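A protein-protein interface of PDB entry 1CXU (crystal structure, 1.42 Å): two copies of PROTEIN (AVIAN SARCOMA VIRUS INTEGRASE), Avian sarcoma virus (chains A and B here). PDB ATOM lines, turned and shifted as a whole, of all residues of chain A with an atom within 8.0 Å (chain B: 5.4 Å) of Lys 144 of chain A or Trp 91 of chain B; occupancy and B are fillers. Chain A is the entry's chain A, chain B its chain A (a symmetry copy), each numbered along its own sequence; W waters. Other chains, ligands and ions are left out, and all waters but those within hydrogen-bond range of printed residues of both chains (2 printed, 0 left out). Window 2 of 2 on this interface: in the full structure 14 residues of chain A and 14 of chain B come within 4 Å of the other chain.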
ATOM      1  N   VAL A  43     -28.200 -11.936  20.142  1.00  0.00           N
ATOM      2  CA  VAL A  43     -27.973 -12.272  21.552  1.00  0.00           C
ATOM      3  C   VAL A  43     -29.170 -11.813  22.378  1.00  0.00           C
ATOM      4  O   VAL A  43     -29.739 -10.728  22.188  1.00  0.00           O
ATOM      5  CB  VAL A  43     -26.656 -11.669  22.104  1.00  0.00           C
ATOM      6  CG1 VAL A  43     -26.645 -10.161  21.948  1.00  0.00           C
ATOM      7  CG2 VAL A  43     -26.455 -12.066  23.559  1.00  0.00           C
ATOM      8  N   LEU A 116     -18.637 -10.952  21.814  1.00  0.00           N
ATOM      9  CA  LEU A 116     -19.661 -10.286  22.626  1.00  0.00           C
ATOM     10  C   LEU A 116     -19.190  -9.876  24.003  1.00  0.00           C
ATOM     11  O   LEU A 116     -19.466  -8.772  24.522  1.00  0.00           O
ATOM     12  CB  LEU A 116     -20.859 -11.250  22.734  1.00  0.00           C
ATOM     13  CG  LEU A 116     -22.043 -10.811  23.589  1.00  0.00           C
ATOM     14  CD1 LEU A 116     -22.689  -9.543  23.050  1.00  0.00           C
ATOM     15  CD2 LEU A 116     -23.081 -11.928  23.688  1.00  0.00           C
ATOM     16  N   LYS A 119     -16.901  -6.889  23.798  1.00  0.00           N
ATOM     17  CA  LYS A 119     -17.611  -5.640  23.492  1.00  0.00           C
ATOM     18  C   LYS A 119     -18.425  -5.137  24.667  1.00  0.00           C
ATOM     19  O   LYS A 119     -18.488  -3.944  24.961  1.00  0.00           O
ATOM     20  CB  LYS A 119     -18.537  -5.858  22.290  1.00  0.00           C
ATOM     21  CG  LYS A 119     -19.275  -4.620  21.796  1.00  0.00           C
ATOM     22  CD  LYS A 119     -18.412  -3.460  21.292  1.00  0.00           C
ATOM     23  CE  LYS A 119     -17.633  -3.847  20.041  1.00  0.00           C
ATOM     24  NZ  LYS A 119     -16.824  -2.650  19.585  1.00  0.00           N
ATOM     25  N   ILE A 120     -19.140  -6.030  25.385  1.00  0.00           N
ATOM     26  CA  ILE A 120     -19.907  -5.651  26.573  1.00  0.00           C
ATOM     27  C   ILE A 120     -19.008  -4.980  27.605  1.00  0.00           C
ATOM     28  O   ILE A 120     -19.347  -3.916  28.172  1.00  0.00           O
ATOM     29  CB  ILE A 120     -20.696  -6.878  27.122  1.00  0.00           C
ATOM     30  CG1 ILE A 120     -21.836  -7.297  26.158  1.00  0.00           C
ATOM     31  CG2 ILE A 120     -21.173  -6.603  28.509  1.00  0.00           C
ATOM     32  CD1 ILE A 120     -22.443  -8.670  26.454  1.00  0.00           C
ATOM     33  N   LEU A 123     -17.933  -1.342  26.316  1.00  0.00           N
ATOM     34  CA  LEU A 123     -19.032  -0.376  26.447  1.00  0.00           C
ATOM     35  C   LEU A 123     -19.331  -0.036  27.884  1.00  0.00           C
ATOM     36  O   LEU A 123     -19.527   1.105  28.277  1.00  0.00           O
ATOM     37  CB  LEU A 123     -20.267  -0.953  25.737  1.00  0.00           C
ATOM     38  CG  LEU A 123     -20.191  -1.163  24.256  1.00  0.00           C
ATOM     39  CD1 LEU A 123     -21.512  -1.776  23.717  1.00  0.00           C
ATOM     40  CD2 LEU A 123     -19.951   0.146  23.482  1.00  0.00           C
ATOM     41  N   ALA A 124     -19.355  -1.099  28.720  1.00  0.00           N
ATOM     42  CA  ALA A 124     -19.658  -0.864  30.122  1.00  0.00           C
ATOM     43  C   ALA A 124     -18.619   0.024  30.845  1.00  0.00           C
ATOM     44  O   ALA A 124     -19.076   0.955  31.496  1.00  0.00           O
ATOM     45  CB  ALA A 124     -19.817  -2.209  30.837  1.00  0.00           C
ATOM     46  N   ASP A 127     -18.960   3.625  30.018  1.00  0.00           N
ATOM     47  CA  ASP A 127     -20.038   4.322  30.694  1.00  0.00           C
ATOM     48  C   ASP A 127     -19.766   4.415  32.198  1.00  0.00           C
ATOM     49  O   ASP A 127     -20.692   4.847  32.930  1.00  0.00           O
ATOM     50  CB  ASP A 127     -21.359   3.539  30.475  1.00  0.00           C
ATOM     51  CG  ASP A 127     -21.953   3.703  29.103  1.00  0.00           C
ATOM     52  OD1 ASP A 127     -21.615   4.705  28.364  1.00  0.00           O
ATOM     53  OD2 ASP A 127     -22.776   2.829  28.718  1.00  0.00           O
ATOM     54  N   LYS A 137     -29.936  -0.243  32.631  1.00  0.00           N
ATOM     55  CA  LYS A 137     -29.092   0.116  31.491  1.00  0.00           C
ATOM     56  C   LYS A 137     -28.700  -1.056  30.616  1.00  0.00           C
ATOM     57  O   LYS A 137     -28.130  -0.898  29.518  1.00  0.00           O
ATOM     58  CB  LYS A 137     -27.825   0.825  31.966  1.00  0.00           C
ATOM     59  CG  LYS A 137     -28.120   2.010  32.873  1.00  0.00           C
ATOM     60  CD  LYS A 137     -28.762   3.155  32.073  1.00  0.00           C
ATOM     61  CE  LYS A 137     -28.768   4.431  32.932  1.00  0.00           C
ATOM     62  NZ  LYS A 137     -27.477   4.662  33.628  1.00  0.00           N
ATOM     63  N   GLN A 138     -28.978  -2.321  31.075  1.00  0.00           N
ATOM     64  CA  GLN A 138     -28.478  -3.520  30.451  1.00  0.00           C
ATOM     65  C   GLN A 138     -29.050  -3.763  29.048  1.00  0.00           C
ATOM     66  O   GLN A 138     -28.313  -4.136  28.123  1.00  0.00           O
ATOM     67  CB  GLN A 138     -28.803  -4.798  31.300  1.00  0.00           C
ATOM     68  CG  GLN A 138     -27.880  -4.865  32.535  1.00  0.00           C
ATOM     69  CD  GLN A 138     -28.260  -6.021  33.441  1.00  0.00           C
ATOM     70  OE1 GLN A 138     -29.148  -6.822  33.131  1.00  0.00           O
ATOM     71  NE2 GLN A 138     -27.572  -6.092  34.585  1.00  0.00           N
ATOM     72  N   GLY A 139     -30.384  -3.564  28.932  1.00  0.00           N
ATOM     73  CA  GLY A 139     -31.026  -3.873  27.635  1.00  0.00           C
ATOM     74  C   GLY A 139     -30.426  -3.058  26.489  1.00  0.00           C
ATOM     75  O   GLY A 139     -30.115  -3.650  25.452  1.00  0.00           O
ATOM     76  N   GLU A 140     -30.306  -1.770  26.733  1.00  0.00           N
ATOM     77  CA  GLU A 140     -29.782  -0.922  25.665  1.00  0.00           C
ATOM     78  C   GLU A 140     -28.298  -1.195  25.404  1.00  0.00           C
ATOM     79  O   GLU A 140     -27.811  -1.172  24.275  1.00  0.00           O
ATOM     80  CB  GLU A 140     -29.964   0.586  25.937  1.00  0.00           C
ATOM     81  CG  GLU A 140     -31.395   1.055  25.922  1.00  0.00           C
ATOM     82  CD  GLU A 140     -31.589   2.566  25.761  1.00  0.00           C
ATOM     83  OE1 GLU A 140     -30.709   3.242  25.239  1.00  0.00           O
ATOM     84  OE2 GLU A 140     -32.717   2.983  26.093  1.00  0.00           O
ATOM     85  N   LEU A 141     -27.536  -1.527  26.491  1.00  0.00           N
ATOM     86  CA  LEU A 141     -26.116  -1.813  26.272  1.00  0.00           C
ATOM     87  C   LEU A 141     -25.914  -3.094  25.437  1.00  0.00           C
ATOM     88  O   LEU A 141     -25.076  -3.205  24.548  1.00  0.00           O
ATOM     89  CB  LEU A 141     -25.342  -1.813  27.618  1.00  0.00           C
ATOM     90  CG  LEU A 141     -23.832  -1.846  27.495  1.00  0.00           C
ATOM     91  CD1 LEU A 141     -23.231  -1.191  28.743  1.00  0.00           C
ATOM     92  CD2 LEU A 141     -23.244  -3.253  27.322  1.00  0.00           C
ATOM     93  N   LEU A 142     -26.713  -4.164  25.747  1.00  0.00           N
ATOM     94  CA  LEU A 142     -26.634  -5.419  25.001  1.00  0.00           C
ATOM     95  C   LEU A 142     -26.982  -5.181  23.531  1.00  0.00           C
ATOM     96  O   LEU A 142     -26.336  -5.719  22.616  1.00  0.00           O
ATOM     97  CB  LEU A 142     -27.572  -6.490  25.637  1.00  0.00           C
ATOM     98  CG  LEU A 142     -27.463  -7.859  25.016  1.00  0.00           C
ATOM     99  CD1 LEU A 142     -26.071  -8.465  25.242  1.00  0.00           C
ATOM    100  CD2 LEU A 142     -28.505  -8.825  25.609  1.00  0.00           C
ATOM    101  N   ALA A 143     -28.031  -4.364  23.305  1.00  0.00           N
ATOM    102  CA  ALA A 143     -28.470  -4.059  21.933  1.00  0.00           C
ATOM    103  C   ALA A 143     -27.414  -3.226  21.210  1.00  0.00           C
ATOM    104  O   ALA A 143     -27.210  -3.438  20.004  1.00  0.00           O
ATOM    105  CB  ALA A 143     -29.811  -3.346  21.953  1.00  0.00           C
ATOM    106  N   LYS A 144     -26.713  -2.339  21.914  1.00  0.00           N
ATOM    107  CA  LYS A 144     -25.605  -1.616  21.292  1.00  0.00           C
ATOM    108  C   LYS A 144     -24.470  -2.551  20.930  1.00  0.00           C
ATOM    109  O   LYS A 144     -23.866  -2.435  19.872  1.00  0.00           O
ATOM    110  CB  LYS A 144     -25.161  -0.514  22.252  1.00  0.00           C
ATOM    111  CG  LYS A 144     -24.084   0.359  21.632  1.00  0.00           C
ATOM    112  CD  LYS A 144     -23.608   1.462  22.599  1.00  0.00           C
ATOM    113  CE  LYS A 144     -24.580   2.599  22.768  1.00  0.00           C
ATOM    114  NZ  LYS A 144     -24.088   3.678  23.696  1.00  0.00           N
ATOM    115  N   ALA A 145     -24.143  -3.539  21.796  1.00  0.00           N
ATOM    116  CA  ALA A 145     -23.090  -4.484  21.464  1.00  0.00           C
ATOM    117  C   ALA A 145     -23.410  -5.310  20.231  1.00  0.00           C
ATOM    118  O   ALA A 145     -22.562  -5.532  19.354  1.00  0.00           O
ATOM    119  CB  ALA A 145     -22.862  -5.402  22.679  1.00  0.00           C
ATOM    120  N   MET A 146     -24.680  -5.747  20.177  1.00  0.00           N
ATOM    121  CA  MET A 146     -25.118  -6.524  18.991  1.00  0.00           C
ATOM    122  C   MET A 146     -25.037  -5.642  17.753  1.00  0.00           C
ATOM    123  O   MET A 146     -24.451  -6.155  16.754  1.00  0.00           O
ATOM    124  CB  MET A 146     -26.533  -7.026  19.273  1.00  0.00           C
ATOM    125  CG  MET A 146     -27.114  -7.844  18.095  1.00  0.00           C
ATOM    126  SD  MET A 146     -28.726  -8.487  18.578  1.00  0.00           S
ATOM    127  CE  MET A 146     -29.418  -8.741  16.930  1.00  0.00           C
ATOM    128  N   TYR A 147     -25.526  -4.423  17.811  1.00  0.00           N
ATOM    129  CA  TYR A 147     -25.376  -3.481  16.673  1.00  0.00           C
ATOM    130  C   TYR A 147     -23.922  -3.336  16.263  1.00  0.00           C
ATOM    131  O   TYR A 147     -23.527  -3.483  15.085  1.00  0.00           O
ATOM    132  CB  TYR A 147     -25.987  -2.134  16.988  1.00  0.00           C
ATOM    133  CG  TYR A 147     -25.542  -0.983  16.100  1.00  0.00           C
ATOM    134  CD1 TYR A 147     -26.047  -0.813  14.806  1.00  0.00           C
ATOM    135  CD2 TYR A 147     -24.595  -0.049  16.514  1.00  0.00           C
ATOM    136  CE1 TYR A 147     -25.624   0.242  13.990  1.00  0.00           C
ATOM    137  CE2 TYR A 147     -24.168   1.012  15.726  1.00  0.00           C
ATOM    138  CZ  TYR A 147     -24.699   1.134  14.467  1.00  0.00           C
ATOM    139  OH  TYR A 147     -24.259   2.212  13.678  1.00  0.00           O
ATOM    140  N   ALA A 148     -23.057  -3.075  17.238  1.00  0.00           N
ATOM    141  CA  ALA A 148     -21.662  -2.824  16.880  1.00  0.00           C
ATOM    142  C   ALA A 148     -21.000  -4.015  16.227  1.00  0.00           C
ATOM    143  O   ALA A 148     -20.165  -3.815  15.324  1.00  0.00           O
ATOM    144  CB  ALA A 148     -20.931  -2.495  18.163  1.00  0.00           C
ATOM    145  N   LEU A 149     -21.299  -5.247  16.626  1.00  0.00           N
ATOM    146  CA  LEU A 149     -20.618  -6.416  16.088  1.00  0.00           C
ATOM    147  C   LEU A 149     -21.136  -6.712  14.688  1.00  0.00           C
ATOM    148  O   LEU A 149     -20.355  -7.183  13.844  1.00  0.00           O
ATOM    149  CB  LEU A 149     -20.765  -7.623  17.006  1.00  0.00           C
ATOM    150  CG  LEU A 149     -20.061  -7.559  18.365  1.00  0.00           C
ATOM    151  CD1 LEU A 149     -20.353  -8.862  19.103  1.00  0.00           C
ATOM    152  CD2 LEU A 149     -18.568  -7.322  18.199  1.00  0.00           C
ATOM    153  N   ASN A 150     -22.394  -6.419  14.436  1.00  0.00           N
ATOM    154  CA  ASN A 150     -23.027  -6.722  13.143  1.00  0.00           C
ATOM    155  C   ASN A 150     -22.745  -5.682  12.069  1.00  0.00           C
ATOM    156  O   ASN A 150     -23.146  -5.796  10.899  1.00  0.00           O
ATOM    157  CB  ASN A 150     -24.540  -6.853  13.332  1.00  0.00           C
ATOM    158  CG  ASN A 150     -24.854  -8.195  14.018  1.00  0.00           C
ATOM    159  OD1 ASN A 150     -24.044  -9.100  13.977  1.00  0.00           O
ATOM    160  ND2 ASN A 150     -26.040  -8.231  14.592  1.00  0.00           N
ATOM    161  N   HIS A 151     -22.085  -4.612  12.459  1.00  0.00           N
ATOM    162  CA  HIS A 151     -21.764  -3.550  11.501  1.00  0.00           C
ATOM    163  C   HIS A 151     -20.379  -3.885  10.963  1.00  0.00           C
ATOM    164  O   HIS A 151     -19.432  -3.875  11.781  1.00  0.00           O
ATOM    165  CB  HIS A 151     -21.856  -2.201  12.201  1.00  0.00           C
ATOM    166  CG  HIS A 151     -21.522  -1.024  11.338  1.00  0.00           C
ATOM    167  ND1 HIS A 151     -20.324  -0.902  10.669  1.00  0.00           N
ATOM    168  CD2 HIS A 151     -22.230   0.092  11.041  1.00  0.00           C
ATOM    169  CE1 HIS A 151     -20.302   0.231   9.992  1.00  0.00           C
ATOM    170  NE2 HIS A 151     -21.452   0.852  10.200  1.00  0.00           N
ATOM    171  N   ILE B  62     -32.537  -0.476  16.376  1.00  0.00           N
ATOM    172  CA  ILE B  62     -31.208  -0.294  15.741  1.00  0.00           C
ATOM    173  C   ILE B  62     -30.480  -1.640  15.618  1.00  0.00           C
ATOM    174  O   ILE B  62     -29.823  -1.914  14.633  1.00  0.00           O
ATOM    175  CB  ILE B  62     -30.450   0.757  16.563  1.00  0.00           C
ATOM    176  CG1 ILE B  62     -31.096   2.145  16.390  1.00  0.00           C
ATOM    177  CG2 ILE B  62     -28.978   0.810  16.224  1.00  0.00           C
ATOM    178  CD1 ILE B  62     -30.537   3.151  17.381  1.00  0.00           C
ATOM    179  N   ARG B  67     -28.706   1.558  12.121  1.00  0.00           N
ATOM    180  CA  ARG B  67     -28.922   2.922  12.590  1.00  0.00           C
ATOM    181  C   ARG B  67     -29.551   3.818  11.511  1.00  0.00           C
ATOM    182  O   ARG B  67     -28.958   3.944  10.431  1.00  0.00           O
ATOM    183  CB  ARG B  67     -27.575   3.544  13.055  1.00  0.00           C
ATOM    184  CG  ARG B  67     -27.871   4.899  13.684  1.00  0.00           C
ATOM    185  CD  ARG B  67     -26.647   5.687  14.084  1.00  0.00           C
ATOM    186  NE  ARG B  67     -25.748   5.885  12.941  1.00  0.00           N
ATOM    187  CZ  ARG B  67     -24.483   6.232  13.235  1.00  0.00           C
ATOM    188  NH1 ARG B  67     -24.165   6.362  14.520  1.00  0.00           N
ATOM    189  NH2 ARG B  67     -23.588   6.436  12.287  1.00  0.00           N
ATOM    190  N   GLU B  86     -32.220  14.586  23.583  1.00  0.00           N
ATOM    191  CA  GLU B  86     -30.816  14.210  23.815  1.00  0.00           C
ATOM    192  C   GLU B  86     -30.420  12.803  23.410  1.00  0.00           C
ATOM    193  O   GLU B  86     -29.306  12.600  22.906  1.00  0.00           O
ATOM    194  CB  GLU B  86     -30.571  14.501  25.304  1.00  0.00           C
ATOM    195  CG  GLU B  86     -29.287  13.972  25.839  1.00  0.00           C
ATOM    196  CD  GLU B  86     -28.045  14.634  25.251  1.00  0.00           C
ATOM    197  OE1 GLU B  86     -28.194  15.658  24.587  1.00  0.00           O
ATOM    198  OE2 GLU B  86     -26.974  14.057  25.542  1.00  0.00           O
ATOM    199  N   TRP B  87     -31.352  11.834  23.595  1.00  0.00           N
ATOM    200  CA  TRP B  87     -31.007  10.431  23.221  1.00  0.00           C
ATOM    201  C   TRP B  87     -30.738  10.326  21.738  1.00  0.00           C
ATOM    202  O   TRP B  87     -29.843   9.717  21.217  1.00  0.00           O
ATOM    203  CB  TRP B  87     -32.153   9.513  23.722  1.00  0.00           C
ATOM    204  CG  TRP B  87     -31.899   8.038  23.561  1.00  0.00           C
ATOM    205  CD1 TRP B  87     -31.457   7.161  24.536  1.00  0.00           C
ATOM    206  CD2 TRP B  87     -32.056   7.212  22.379  1.00  0.00           C
ATOM    207  NE1 TRP B  87     -31.330   5.872  24.051  1.00  0.00           N
ATOM    208  CE2 TRP B  87     -31.700   5.894  22.721  1.00  0.00           C
ATOM    209  CE3 TRP B  87     -32.474   7.438  21.052  1.00  0.00           C
ATOM    210  CZ2 TRP B  87     -31.724   4.797  21.836  1.00  0.00           C
ATOM    211  CZ3 TRP B  87     -32.501   6.373  20.158  1.00  0.00           C
ATOM    212  CH2 TRP B  87     -32.137   5.051  20.529  1.00  0.00           C
ATOM    213  N   LEU B  88     -31.620  10.959  20.938  1.00  0.00           N
ATOM    214  CA  LEU B  88     -31.482  10.979  19.480  1.00  0.00           C
ATOM    215  C   LEU B  88     -30.209  11.707  19.002  1.00  0.00           C
ATOM    216  O   LEU B  88     -29.508  11.241  18.125  1.00  0.00           O
ATOM    217  CB  LEU B  88     -32.721  11.600  18.830  1.00  0.00           C
ATOM    218  CG  LEU B  88     -33.991  10.743  18.967  1.00  0.00           C
ATOM    219  CD1 LEU B  88     -35.217  11.544  18.632  1.00  0.00           C
ATOM    220  CD2 LEU B  88     -33.937   9.520  18.050  1.00  0.00           C
ATOM    221  N   ALA B  89     -29.922  12.820  19.712  1.00  0.00           N
ATOM    222  CA  ALA B  89     -28.660  13.528  19.377  1.00  0.00           C
ATOM    223  C   ALA B  89     -27.435  12.697  19.709  1.00  0.00           C
ATOM    224  O   ALA B  89     -26.447  12.654  18.999  1.00  0.00           O
ATOM    225  CB  ALA B  89     -28.692  14.874  20.130  1.00  0.00           C
ATOM    226  N   ARG B  90     -27.494  11.949  20.840  1.00  0.00           N
ATOM    227  CA  ARG B  90     -26.416  11.033  21.222  1.00  0.00           C
ATOM    228  C   ARG B  90     -26.076  10.020  20.138  1.00  0.00           C
ATOM    229  O   ARG B  90     -24.927   9.636  19.917  1.00  0.00           O
ATOM    230  CB  ARG B  90     -26.756  10.314  22.543  1.00  0.00           C
ATOM    231  CG  ARG B  90     -25.714   9.275  22.932  1.00  0.00           C
ATOM    232  CD  ARG B  90     -26.225   8.262  23.941  1.00  0.00           C
ATOM    233  NE  ARG B  90     -27.229   8.800  24.837  1.00  0.00           N
ATOM    234  CZ  ARG B  90     -28.042   8.123  25.636  1.00  0.00           C
ATOM    235  NH1 ARG B  90     -28.024   6.796  25.714  1.00  0.00           N
ATOM    236  NH2 ARG B  90     -28.909   8.812  26.391  1.00  0.00           N
ATOM    237  N   TRP B  91     -27.149   9.525  19.440  1.00  0.00           N
ATOM    238  CA  TRP B  91     -27.030   8.567  18.373  1.00  0.00           C
ATOM    239  C   TRP B  91     -26.789   9.193  16.987  1.00  0.00           C
ATOM    240  O   TRP B  91     -26.536   8.488  16.015  1.00  0.00           O
ATOM    241  CB  TRP B  91     -28.315   7.706  18.306  1.00  0.00           C
ATOM    242  CG  TRP B  91     -28.260   6.464  19.190  1.00  0.00           C
ATOM    243  CD1 TRP B  91     -28.783   6.331  20.453  1.00  0.00           C
ATOM    244  CD2 TRP B  91     -27.634   5.221  18.841  1.00  0.00           C
ATOM    245  NE1 TRP B  91     -28.508   5.030  20.893  1.00  0.00           N
ATOM    246  CE2 TRP B  91     -27.815   4.323  19.975  1.00  0.00           C
ATOM    247  CE3 TRP B  91     -26.939   4.748  17.732  1.00  0.00           C
ATOM    248  CZ2 TRP B  91     -27.306   3.015  19.941  1.00  0.00           C
ATOM    249  CZ3 TRP B  91     -26.443   3.458  17.699  1.00  0.00           C
ATOM    250  CH2 TRP B  91     -26.639   2.606  18.814  1.00  0.00           C
ATOM    251  N   GLY B  92     -26.839  10.555  16.928  1.00  0.00           N
ATOM    252  CA  GLY B  92     -26.714  11.199  15.615  1.00  0.00           C
ATOM    253  C   GLY B  92     -27.910  10.937  14.675  1.00  0.00           C
ATOM    254  O   GLY B  92     -27.671  10.805  13.480  1.00  0.00           O
ATOM    255  N   ILE B  93     -29.112  10.817  15.227  1.00  0.00           N
ATOM    256  CA  ILE B  93     -30.306  10.555  14.413  1.00  0.00           C
ATOM    257  C   ILE B  93     -31.167  11.794  14.373  1.00  0.00           C
ATOM    258  O   ILE B  93     -31.551  12.348  15.398  1.00  0.00           O
ATOM    259  CB  ILE B  93     -31.069   9.332  15.007  1.00  0.00           C
ATOM    260  CG1 ILE B  93     -30.267   8.029  14.935  1.00  0.00           C
ATOM    261  CG2 ILE B  93     -32.465   9.223  14.354  1.00  0.00           C
ATOM    262  CD1 ILE B  93     -30.847   6.891  15.800  1.00  0.00           C
HETATM  263  O   HOH W   1     -29.287   2.867  23.303  1.00  0.00           O
HETATM  264  O   HOH W   2     -27.137   4.320  24.116  1.00  0.00           O
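The side-chain carboxylate (OE1) of Glu 140 of chain A lies within hydrogen-bond range of the indole nitrogen (NE1) of Trp 87 of chain B (3.0 Å).
Among the printed residues, pairs that only touch across the chains: Tyr 147 of chain A with Arg 67 of chain B, Tyr 147 of chain A with Ile 62 of chain B, Tyr 147 of chain A with Trp 91 of chain B and Lys 144 of chain A with Trp 91 of chain B.
Of chain B, only Trp 91 comes within 4 Å of Lys 144 of chain A. Trp 91 of chain B touches two residues of chain A. Gly 92 of chain B touches none of the printed residues of chain A. Of the printed residues of chain B, Glu 140 of chain A touches Trp 87 (3.0 Å). Of the printed residues of chain B, Tyr 147 of chain A touches Ile 62 (3.6 Å), Arg 67 (3.6 Å) and Trp 91 (3.9 Å). Of the printed residues of chain A, Ile 62 of chain B touches Tyr 147 (3.6 Å). Printed residues of chain A within 4 Å of Arg 67 of chain B: Tyr 147 (3.6 Å). The nearest residue of chain A that does not touch Trp 91 of chain B is Glu 140 of chain A (5.2 Å). The nearest printed residue of chain B that does not touch Glu 140 of chain A is Arg 90 of chain B (4.5 Å).
Printed residues of chain A that touch a printed residue of chain B: Glu 140, Lys 144 and Tyr 147. Hydrophobic or aromatic side chains of chain A that line the printed part of chain B: Tyr 147. Of the 10 printed residues of chain B, 4 touch a printed residue of chain A. Printed residues of chain B that touch a printed residue of chain A: Ile 62, Arg 67, Trp 87 and Trp 91. Along chain B the printed residues that touch a printed residue of chain A span positions 62 to 91. Among the printed residues, 5 pairs touch across the chains. Among the printed residues, no Asp or Glu carboxylate lies within 4 Å of a Lys or Arg side-chain nitrogen of the other chain.
No position is printed for both chains.
Water W1 bridges OE1 of Glu 140 of chain A and NE1 of Trp 91 of chain B. Water W2 bridges NH1 of Arg 90 of chain B (3.1 Å) and NZ of Lys 144 of chain A (3.1 Å).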
